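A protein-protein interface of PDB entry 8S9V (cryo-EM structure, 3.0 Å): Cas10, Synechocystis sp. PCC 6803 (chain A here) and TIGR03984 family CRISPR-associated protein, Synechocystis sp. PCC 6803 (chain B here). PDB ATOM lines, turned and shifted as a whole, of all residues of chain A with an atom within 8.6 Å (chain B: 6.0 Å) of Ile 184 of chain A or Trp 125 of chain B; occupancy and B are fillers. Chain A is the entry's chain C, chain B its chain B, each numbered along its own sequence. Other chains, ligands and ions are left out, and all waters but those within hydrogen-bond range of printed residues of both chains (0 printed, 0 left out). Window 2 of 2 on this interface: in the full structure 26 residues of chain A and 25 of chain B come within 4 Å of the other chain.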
ATOM      1  N   ARG A 181     -23.630  11.273  19.025  1.00  0.00           N
ATOM      2  CA  ARG A 181     -24.128  10.020  19.573  1.00  0.00           C
ATOM      3  C   ARG A 181     -24.793   9.131  18.538  1.00  0.00           C
ATOM      4  O   ARG A 181     -25.663   9.574  17.786  1.00  0.00           O
ATOM      5  CB  ARG A 181     -25.133  10.296  20.666  1.00  0.00           C
ATOM      6  CG  ARG A 181     -25.699   9.043  21.198  1.00  0.00           C
ATOM      7  CD  ARG A 181     -24.788   8.432  22.162  1.00  0.00           C
ATOM      8  NE  ARG A 181     -24.770   9.218  23.365  1.00  0.00           N
ATOM      9  CZ  ARG A 181     -24.889   8.689  24.566  1.00  0.00           C
ATOM     10  NH1 ARG A 181     -25.029   9.453  25.624  1.00  0.00           N
ATOM     11  NH2 ARG A 181     -24.983   7.383  24.682  1.00  0.00           N
ATOM     12  N   LEU A 182     -24.343   7.863  18.476  1.00  0.00           N
ATOM     13  CA  LEU A 182     -25.149   6.761  17.977  1.00  0.00           C
ATOM     14  C   LEU A 182     -25.907   6.125  19.130  1.00  0.00           C
ATOM     15  O   LEU A 182     -25.443   6.149  20.264  1.00  0.00           O
ATOM     16  CB  LEU A 182     -24.280   5.708  17.326  1.00  0.00           C
ATOM     17  CG  LEU A 182     -23.648   6.061  16.002  1.00  0.00           C
ATOM     18  CD1 LEU A 182     -22.180   6.015  16.190  1.00  0.00           C
ATOM     19  CD2 LEU A 182     -24.071   5.054  14.985  1.00  0.00           C
ATOM     20  N   PRO A 183     -27.084   5.569  18.903  1.00  0.00           N
ATOM     21  CA  PRO A 183     -27.852   5.033  20.029  1.00  0.00           C
ATOM     22  C   PRO A 183     -27.091   4.030  20.862  1.00  0.00           C
ATOM     23  O   PRO A 183     -27.259   3.989  22.079  1.00  0.00           O
ATOM     24  CB  PRO A 183     -29.031   4.374  19.325  1.00  0.00           C
ATOM     25  CG  PRO A 183     -29.205   5.158  18.135  1.00  0.00           C
ATOM     26  CD  PRO A 183     -27.841   5.469  17.654  1.00  0.00           C
ATOM     27  N   ILE A 184     -26.244   3.216  20.224  1.00  0.00           N
ATOM     28  CA  ILE A 184     -25.521   2.110  20.854  1.00  0.00           C
ATOM     29  C   ILE A 184     -24.280   2.491  21.645  1.00  0.00           C
ATOM     30  O   ILE A 184     -23.638   1.599  22.197  1.00  0.00           O
ATOM     31  CB  ILE A 184     -25.149   1.077  19.781  1.00  0.00           C
ATOM     32  CG1 ILE A 184     -24.201   1.691  18.775  1.00  0.00           C
ATOM     33  CG2 ILE A 184     -26.376   0.636  19.066  1.00  0.00           C
ATOM     34  CD1 ILE A 184     -23.628   0.699  17.821  1.00  0.00           C
ATOM     35  N   ALA A 185     -23.906   3.760  21.727  1.00  0.00           N
ATOM     36  CA  ALA A 185     -22.645   4.161  22.329  1.00  0.00           C
ATOM     37  C   ALA A 185     -22.858   4.671  23.745  1.00  0.00           C
ATOM     38  O   ALA A 185     -23.742   5.489  23.986  1.00  0.00           O
ATOM     39  CB  ALA A 185     -21.988   5.242  21.479  1.00  0.00           C
ATOM     40  N   ALA A 186     -22.017   4.216  24.667  1.00  0.00           N
ATOM     41  CA  ALA A 186     -22.131   4.531  26.081  1.00  0.00           C
ATOM     42  C   ALA A 186     -21.836   5.998  26.353  1.00  0.00           C
ATOM     43  O   ALA A 186     -21.364   6.728  25.489  1.00  0.00           O
ATOM     44  CB  ALA A 186     -21.204   3.643  26.895  1.00  0.00           C
ATOM     45  N   GLY A 187     -22.166   6.442  27.574  1.00  0.00           N
ATOM     46  CA  GLY A 187     -22.021   7.826  27.975  1.00  0.00           C
ATOM     47  C   GLY A 187     -20.745   8.156  28.742  1.00  0.00           C
ATOM     48  O   GLY A 187     -20.103   7.293  29.316  1.00  0.00           O
ATOM     49  N   CYS A 188     -20.391   9.443  28.736  1.00  0.00           N
ATOM     50  CA  CYS A 188     -19.124   9.979  29.229  1.00  0.00           C
ATOM     51  C   CYS A 188     -18.956  10.022  30.749  1.00  0.00           C
ATOM     52  O   CYS A 188     -17.901  10.467  31.190  1.00  0.00           O
ATOM     53  CB  CYS A 188     -18.906  11.378  28.672  1.00  0.00           C
ATOM     54  SG  CYS A 188     -17.320  12.117  29.054  1.00  0.00           S
ATOM     55  N   PRO A 194     -20.794  10.913  23.913  1.00  0.00           N
ATOM     56  CA  PRO A 194     -20.576   9.474  24.023  1.00  0.00           C
ATOM     57  C   PRO A 194     -19.178   9.143  24.499  1.00  0.00           C
ATOM     58  O   PRO A 194     -18.201   9.760  24.082  1.00  0.00           O
ATOM     59  CB  PRO A 194     -20.806   8.984  22.598  1.00  0.00           C
ATOM     60  CG  PRO A 194     -20.456  10.094  21.787  1.00  0.00           C
ATOM     61  CD  PRO A 194     -20.887  11.318  22.511  1.00  0.00           C
ATOM     62  N   ALA A 195     -19.089   8.137  25.357  1.00  0.00           N
ATOM     63  CA  ALA A 195     -17.808   7.674  25.856  1.00  0.00           C
ATOM     64  C   ALA A 195     -16.996   7.052  24.747  1.00  0.00           C
ATOM     65  O   ALA A 195     -17.535   6.552  23.763  1.00  0.00           O
ATOM     66  CB  ALA A 195     -17.997   6.666  26.978  1.00  0.00           C
ATOM     67  N   PRO A 208     -15.643   5.286  32.204  1.00  0.00           N
ATOM     68  CA  PRO A 208     -15.637   5.765  30.821  1.00  0.00           C
ATOM     69  C   PRO A 208     -15.575   7.277  30.762  1.00  0.00           C
ATOM     70  O   PRO A 208     -16.122   7.970  31.616  1.00  0.00           O
ATOM     71  CB  PRO A 208     -16.962   5.255  30.257  1.00  0.00           C
ATOM     72  CG  PRO A 208     -17.473   4.312  31.247  1.00  0.00           C
ATOM     73  CD  PRO A 208     -16.946   4.726  32.562  1.00  0.00           C
ATOM     74  N   LEU B  38     -27.509  -0.444  10.857  1.00  0.00           N
ATOM     75  CA  LEU B  38     -28.163   0.112  12.029  1.00  0.00           C
ATOM     76  C   LEU B  38     -29.445   0.774  11.556  1.00  0.00           C
ATOM     77  O   LEU B  38     -29.402   1.829  10.926  1.00  0.00           O
ATOM     78  CB  LEU B  38     -27.242   1.083  12.751  1.00  0.00           C
ATOM     79  CG  LEU B  38     -27.692   1.801  14.005  1.00  0.00           C
ATOM     80  CD1 LEU B  38     -28.059   0.843  15.086  1.00  0.00           C
ATOM     81  CD2 LEU B  38     -26.525   2.626  14.454  1.00  0.00           C
ATOM     82  N   CYS B  45     -34.469  -0.039  17.501  1.00  0.00           N
ATOM     83  CA  CYS B  45     -33.240   0.221  16.759  1.00  0.00           C
ATOM     84  C   CYS B  45     -32.453  -1.075  16.621  1.00  0.00           C
ATOM     85  O   CYS B  45     -32.021  -1.654  17.619  1.00  0.00           O
ATOM     86  CB  CYS B  45     -32.410   1.277  17.480  1.00  0.00           C
ATOM     87  SG  CYS B  45     -30.750   1.529  16.889  1.00  0.00           S
ATOM     88  N   LEU B  47     -29.451  -3.530  15.080  1.00  0.00           N
ATOM     89  CA  LEU B  47     -28.259  -3.916  14.351  1.00  0.00           C
ATOM     90  C   LEU B  47     -28.587  -5.057  13.405  1.00  0.00           C
ATOM     91  O   LEU B  47     -29.383  -5.936  13.727  1.00  0.00           O
ATOM     92  CB  LEU B  47     -27.154  -4.315  15.315  1.00  0.00           C
ATOM     93  CG  LEU B  47     -26.414  -3.140  15.940  1.00  0.00           C
ATOM     94  CD1 LEU B  47     -25.591  -3.583  17.117  1.00  0.00           C
ATOM     95  CD2 LEU B  47     -25.510  -2.534  14.904  1.00  0.00           C
ATOM     96  N   LEU B 123     -17.345   3.760  22.620  1.00  0.00           N
ATOM     97  CA  LEU B 123     -17.559   2.595  23.459  1.00  0.00           C
ATOM     98  C   LEU B 123     -19.007   2.129  23.384  1.00  0.00           C
ATOM     99  O   LEU B 123     -19.913   2.903  23.682  1.00  0.00           O
ATOM    100  CB  LEU B 123     -17.191   2.980  24.881  1.00  0.00           C
ATOM    101  CG  LEU B 123     -17.314   2.047  26.050  1.00  0.00           C
ATOM    102  CD1 LEU B 123     -16.339   0.968  25.858  1.00  0.00           C
ATOM    103  CD2 LEU B 123     -17.001   2.827  27.266  1.00  0.00           C
ATOM    104  N   LEU B 124     -19.243   0.874  23.000  1.00  0.00           N
ATOM    105  CA  LEU B 124     -20.598   0.331  23.021  1.00  0.00           C
ATOM    106  C   LEU B 124     -21.049   0.017  24.444  1.00  0.00           C
ATOM    107  O   LEU B 124     -20.247  -0.184  25.346  1.00  0.00           O
ATOM    108  CB  LEU B 124     -20.727  -0.915  22.164  1.00  0.00           C
ATOM    109  CG  LEU B 124     -20.397  -0.815  20.691  1.00  0.00           C
ATOM    110  CD1 LEU B 124     -20.962  -1.980  19.971  1.00  0.00           C
ATOM    111  CD2 LEU B 124     -20.919   0.440  20.124  1.00  0.00           C
ATOM    112  N   TRP B 125     -22.362  -0.047  24.625  1.00  0.00           N
ATOM    113  CA  TRP B 125     -22.962  -0.353  25.918  1.00  0.00           C
ATOM    114  C   TRP B 125     -22.569  -1.711  26.477  1.00  0.00           C
ATOM    115  O   TRP B 125     -22.764  -2.741  25.835  1.00  0.00           O
ATOM    116  CB  TRP B 125     -24.480  -0.328  25.806  1.00  0.00           C
ATOM    117  CG  TRP B 125     -25.136   0.963  25.599  1.00  0.00           C
ATOM    118  CD1 TRP B 125     -25.778   1.374  24.485  1.00  0.00           C
ATOM    119  CD2 TRP B 125     -25.302   1.997  26.558  1.00  0.00           C
ATOM    120  NE1 TRP B 125     -26.309   2.615  24.675  1.00  0.00           N
ATOM    121  CE2 TRP B 125     -26.022   3.019  25.948  1.00  0.00           C
ATOM    122  CE3 TRP B 125     -24.893   2.164  27.872  1.00  0.00           C
ATOM    123  CZ2 TRP B 125     -26.335   4.183  26.601  1.00  0.00           C
ATOM    124  CZ3 TRP B 125     -25.200   3.315  28.505  1.00  0.00           C
ATOM    125  CH2 TRP B 125     -25.916   4.310  27.879  1.00  0.00           C
ATOM    126  N   GLY B 126     -22.070  -1.713  27.700  1.00  0.00           N
ATOM    127  CA  GLY B 126     -21.986  -2.914  28.501  1.00  0.00           C
ATOM    128  C   GLY B 126     -20.806  -3.835  28.251  1.00  0.00           C
ATOM    129  O   GLY B 126     -20.005  -3.673  27.333  1.00  0.00           O
ATOM    130  N   GLU B 127     -20.718  -4.825  29.123  1.00  0.00           N
ATOM    131  CA  GLU B 127     -19.725  -5.881  29.150  1.00  0.00           C
ATOM    132  C   GLU B 127     -20.294  -7.140  28.535  1.00  0.00           C
ATOM    133  O   GLU B 127     -21.505  -7.262  28.354  1.00  0.00           O
ATOM    134  CB  GLU B 127     -19.286  -6.128  30.591  1.00  0.00           C
ATOM    135  CG  GLU B 127     -19.030  -4.844  31.345  1.00  0.00           C
ATOM    136  CD  GLU B 127     -18.178  -5.027  32.574  1.00  0.00           C
ATOM    137  OE1 GLU B 127     -16.998  -5.381  32.428  1.00  0.00           O
ATOM    138  OE2 GLU B 127     -18.669  -4.772  33.691  1.00  0.00           O
ATOM    139  N   LEU B 141     -23.574  -8.161  24.500  1.00  0.00           N
ATOM    140  CA  LEU B 141     -23.193  -7.261  25.569  1.00  0.00           C
ATOM    141  C   LEU B 141     -24.379  -7.107  26.503  1.00  0.00           C
ATOM    142  O   LEU B 141     -25.521  -7.311  26.109  1.00  0.00           O
ATOM    143  CB  LEU B 141     -22.789  -5.912  24.995  1.00  0.00           C
ATOM    144  CG  LEU B 141     -21.708  -5.933  23.934  1.00  0.00           C
ATOM    145  CD1 LEU B 141     -21.481  -4.558  23.478  1.00  0.00           C
ATOM    146  CD2 LEU B 141     -20.462  -6.467  24.512  1.00  0.00           C
ATOM    147  N   ALA B 142     -24.117  -6.721  27.743  1.00  0.00           N
ATOM    148  CA  ALA B 142     -25.222  -6.438  28.641  1.00  0.00           C
ATOM    149  C   ALA B 142     -24.819  -5.372  29.634  1.00  0.00           C
ATOM    150  O   ALA B 142     -23.688  -5.363  30.109  1.00  0.00           O
ATOM    151  CB  ALA B 142     -25.662  -7.689  29.383  1.00  0.00           C
ATOM    152  N   GLU B 143     -25.772  -4.516  29.982  1.00  0.00           N
ATOM    153  CA  GLU B 143     -25.637  -3.571  31.077  1.00  0.00           C
ATOM    154  C   GLU B 143     -26.959  -3.391  31.789  1.00  0.00           C
ATOM    155  O   GLU B 143     -28.002  -3.317  31.145  1.00  0.00           O
ATOM    156  CB  GLU B 143     -25.194  -2.209  30.597  1.00  0.00           C
ATOM    157  CG  GLU B 143     -25.060  -1.293  31.749  1.00  0.00           C
ATOM    158  CD  GLU B 143     -24.384  -0.013  31.415  1.00  0.00           C
ATOM    159  OE1 GLU B 143     -23.884   0.108  30.284  1.00  0.00           O
ATOM    160  OE2 GLU B 143     -24.331   0.863  32.303  1.00  0.00           O
ATOM    161  N   ARG B 145     -28.301  -0.955  33.043  1.00  0.00           N
ATOM    162  CA  ARG B 145     -28.986   0.236  32.558  1.00  0.00           C
ATOM    163  C   ARG B 145     -29.910  -0.015  31.381  1.00  0.00           C
ATOM    164  O   ARG B 145     -30.916   0.674  31.234  1.00  0.00           O
ATOM    165  CB  ARG B 145     -27.943   1.254  32.160  1.00  0.00           C
ATOM    166  CG  ARG B 145     -28.482   2.563  31.916  1.00  0.00           C
ATOM    167  CD  ARG B 145     -27.377   3.505  31.710  1.00  0.00           C
ATOM    168  NE  ARG B 145     -27.910   4.835  31.571  1.00  0.00           N
ATOM    169  CZ  ARG B 145     -27.157   5.910  31.571  1.00  0.00           C
ATOM    170  NH1 ARG B 145     -27.699   7.108  31.481  1.00  0.00           N
ATOM    171  NH2 ARG B 145     -25.853   5.772  31.680  1.00  0.00           N
ATOM    172  N   ILE B 146     -29.586  -0.969  30.512  1.00  0.00           N
ATOM    173  CA  ILE B 146     -30.300  -1.148  29.256  1.00  0.00           C
ATOM    174  C   ILE B 146     -30.658  -2.596  28.979  1.00  0.00           C
ATOM    175  O   ILE B 146     -31.359  -2.873  28.013  1.00  0.00           O
ATOM    176  CB  ILE B 146     -29.508  -0.550  28.072  1.00  0.00           C
ATOM    177  CG1 ILE B 146     -28.194  -1.275  27.860  1.00  0.00           C
ATOM    178  CG2 ILE B 146     -29.224   0.905  28.291  1.00  0.00           C
ATOM    179  CD1 ILE B 146     -27.927  -1.577  26.454  1.00  0.00           C
ATOM    180  N   LEU B 149     -27.545  -6.084  24.688  1.00  0.00           N
ATOM    181  CA  LEU B 149     -27.388  -5.598  23.321  1.00  0.00           C
ATOM    182  C   LEU B 149     -26.687  -6.691  22.527  1.00  0.00           C
ATOM    183  O   LEU B 149     -25.506  -6.938  22.753  1.00  0.00           O
ATOM    184  CB  LEU B 149     -26.583  -4.298  23.297  1.00  0.00           C
ATOM    185  CG  LEU B 149     -26.238  -3.607  21.973  1.00  0.00           C
ATOM    186  CD1 LEU B 149     -27.472  -3.068  21.313  1.00  0.00           C
ATOM    187  CD2 LEU B 149     -25.225  -2.508  22.157  1.00  0.00           C
ATOM    188  N   VAL B 163     -16.287  -3.562  23.470  1.00  0.00           N
ATOM    189  CA  VAL B 163     -16.389  -3.379  22.034  1.00  0.00           C
ATOM    190  C   VAL B 163     -16.448  -1.891  21.744  1.00  0.00           C
ATOM    191  O   VAL B 163     -17.237  -1.168  22.354  1.00  0.00           O
ATOM    192  CB  VAL B 163     -17.613  -4.106  21.471  1.00  0.00           C
ATOM    193  CG1 VAL B 163     -17.652  -3.966  19.987  1.00  0.00           C
ATOM    194  CG2 VAL B 163     -17.550  -5.527  21.856  1.00  0.00           C
ATOM    195  N   LEU B 165     -17.040   0.693  18.554  1.00  0.00           N
ATOM    196  CA  LEU B 165     -17.207   1.100  17.170  1.00  0.00           C
ATOM    197  C   LEU B 165     -16.097   2.079  16.798  1.00  0.00           C
ATOM    198  O   LEU B 165     -15.710   2.922  17.603  1.00  0.00           O
ATOM    199  CB  LEU B 165     -18.589   1.703  16.978  1.00  0.00           C
ATOM    200  CG  LEU B 165     -18.966   2.343  15.661  1.00  0.00           C
ATOM    201  CD1 LEU B 165     -18.960   1.272  14.628  1.00  0.00           C
ATOM    202  CD2 LEU B 165     -20.332   2.935  15.762  1.00  0.00           C
ATOM    203  N   LEU B 190     -16.822  -2.659  14.130  1.00  0.00           N
ATOM    204  CA  LEU B 190     -16.718  -2.959  15.547  1.00  0.00           C
ATOM    205  C   LEU B 190     -15.381  -3.600  15.861  1.00  0.00           C
ATOM    206  O   LEU B 190     -14.942  -4.524  15.177  1.00  0.00           O
ATOM    207  CB  LEU B 190     -17.842  -3.902  15.959  1.00  0.00           C
ATOM    208  CG  LEU B 190     -19.280  -3.438  15.779  1.00  0.00           C
ATOM    209  CD1 LEU B 190     -20.195  -4.440  16.385  1.00  0.00           C
ATOM    210  CD2 LEU B 190     -19.483  -2.125  16.445  1.00  0.00           C
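Of the printed residues of chain B, Leu 182 of chain A touches Leu 38 (3.5 Å) and Leu 165 (3.6 Å). Printed residues of chain B within 4 Å of Pro 183 of chain A: Trp 125 (3.1 Å). Printed residues of chain B within 4 Å of Ala 195 of chain A: Leu 123 (3.0 Å). Trp 125 of chain B touches just these residues of chain A: Arg 181, Pro 183, Ile 184 and Ala 185. Leu 141 of chain B touches none of the printed residues of chain A. The nearest residue of chain A that does not touch Trp 125 of chain B is Ala 186 of chain A (4.1 Å).
The backbone NH of Leu 123 of chain B sits at hydrogen-bond distance from the backbone carbonyl oxygen of Ala 195 of chain A (3.0 Å). O of Pro 183 of chain A sits at hydrogen-bond distance from NE1 of Trp 125 of chain B (3.1 Å). The backbone NH (N) of Ala 186 of chain A lies within hydrogen-bond range of the backbone carbonyl oxygen (O) of Leu 123 of chain B (2.7 Å). The backbone carbonyl oxygen (O) of Ile 184 of chain A lies close to the backbone NH (N) of Trp 125 of chain B (3.2 Å).
Hydrophobic or aromatic side chains of chain A within 4 Å of the printed part of chain B: Leu 182, Ile 184, Ala 185, Ala 186, Ala 195 and Pro 208. Printed residues of chain B that touch a printed residue of chain A: Leu 38, Leu 123, Leu 124, Trp 125 and Leu 165. Hydrophobic or aromatic side chains of chain B within 4 Å of the printed part of chain A: Leu 38, Leu 123, Leu 124, Trp 125 and Leu 165. Among the printed residues, 11 pairs touch across the chains. Among the printed residues, no Asp or Glu carboxylate lies within 4 Å of a Lys or Arg side-chain nitrogen of the other chain.
Among the printed residues, pairs that only touch across the chains: Ala 185 of chain A with Leu 123 of chain B, Ile 184 of chain A with Leu 124 of chain B, Leu 182 of chain A with Leu 38 of chain B, Leu 182 of chain A with Leu 165 of chain B, Pro 208 of chain A with Leu 123 of chain B, Ala 185 of chain A with Trp 125 of chain B and Arg 181 of chain A with Trp 125 of chain B.
The backbone carbonyl oxygen (O) of Ala 186 of chain A sits at hydrogen-bond distance from the backbone NH (N) of Ala 195 of chain A (2.7 Å). The backbone NH (N) of Leu 124 of chain B is in hydrogen-bond range of the backbone carbonyl oxygen (O) of Val 163 of chain B (2.9 Å).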
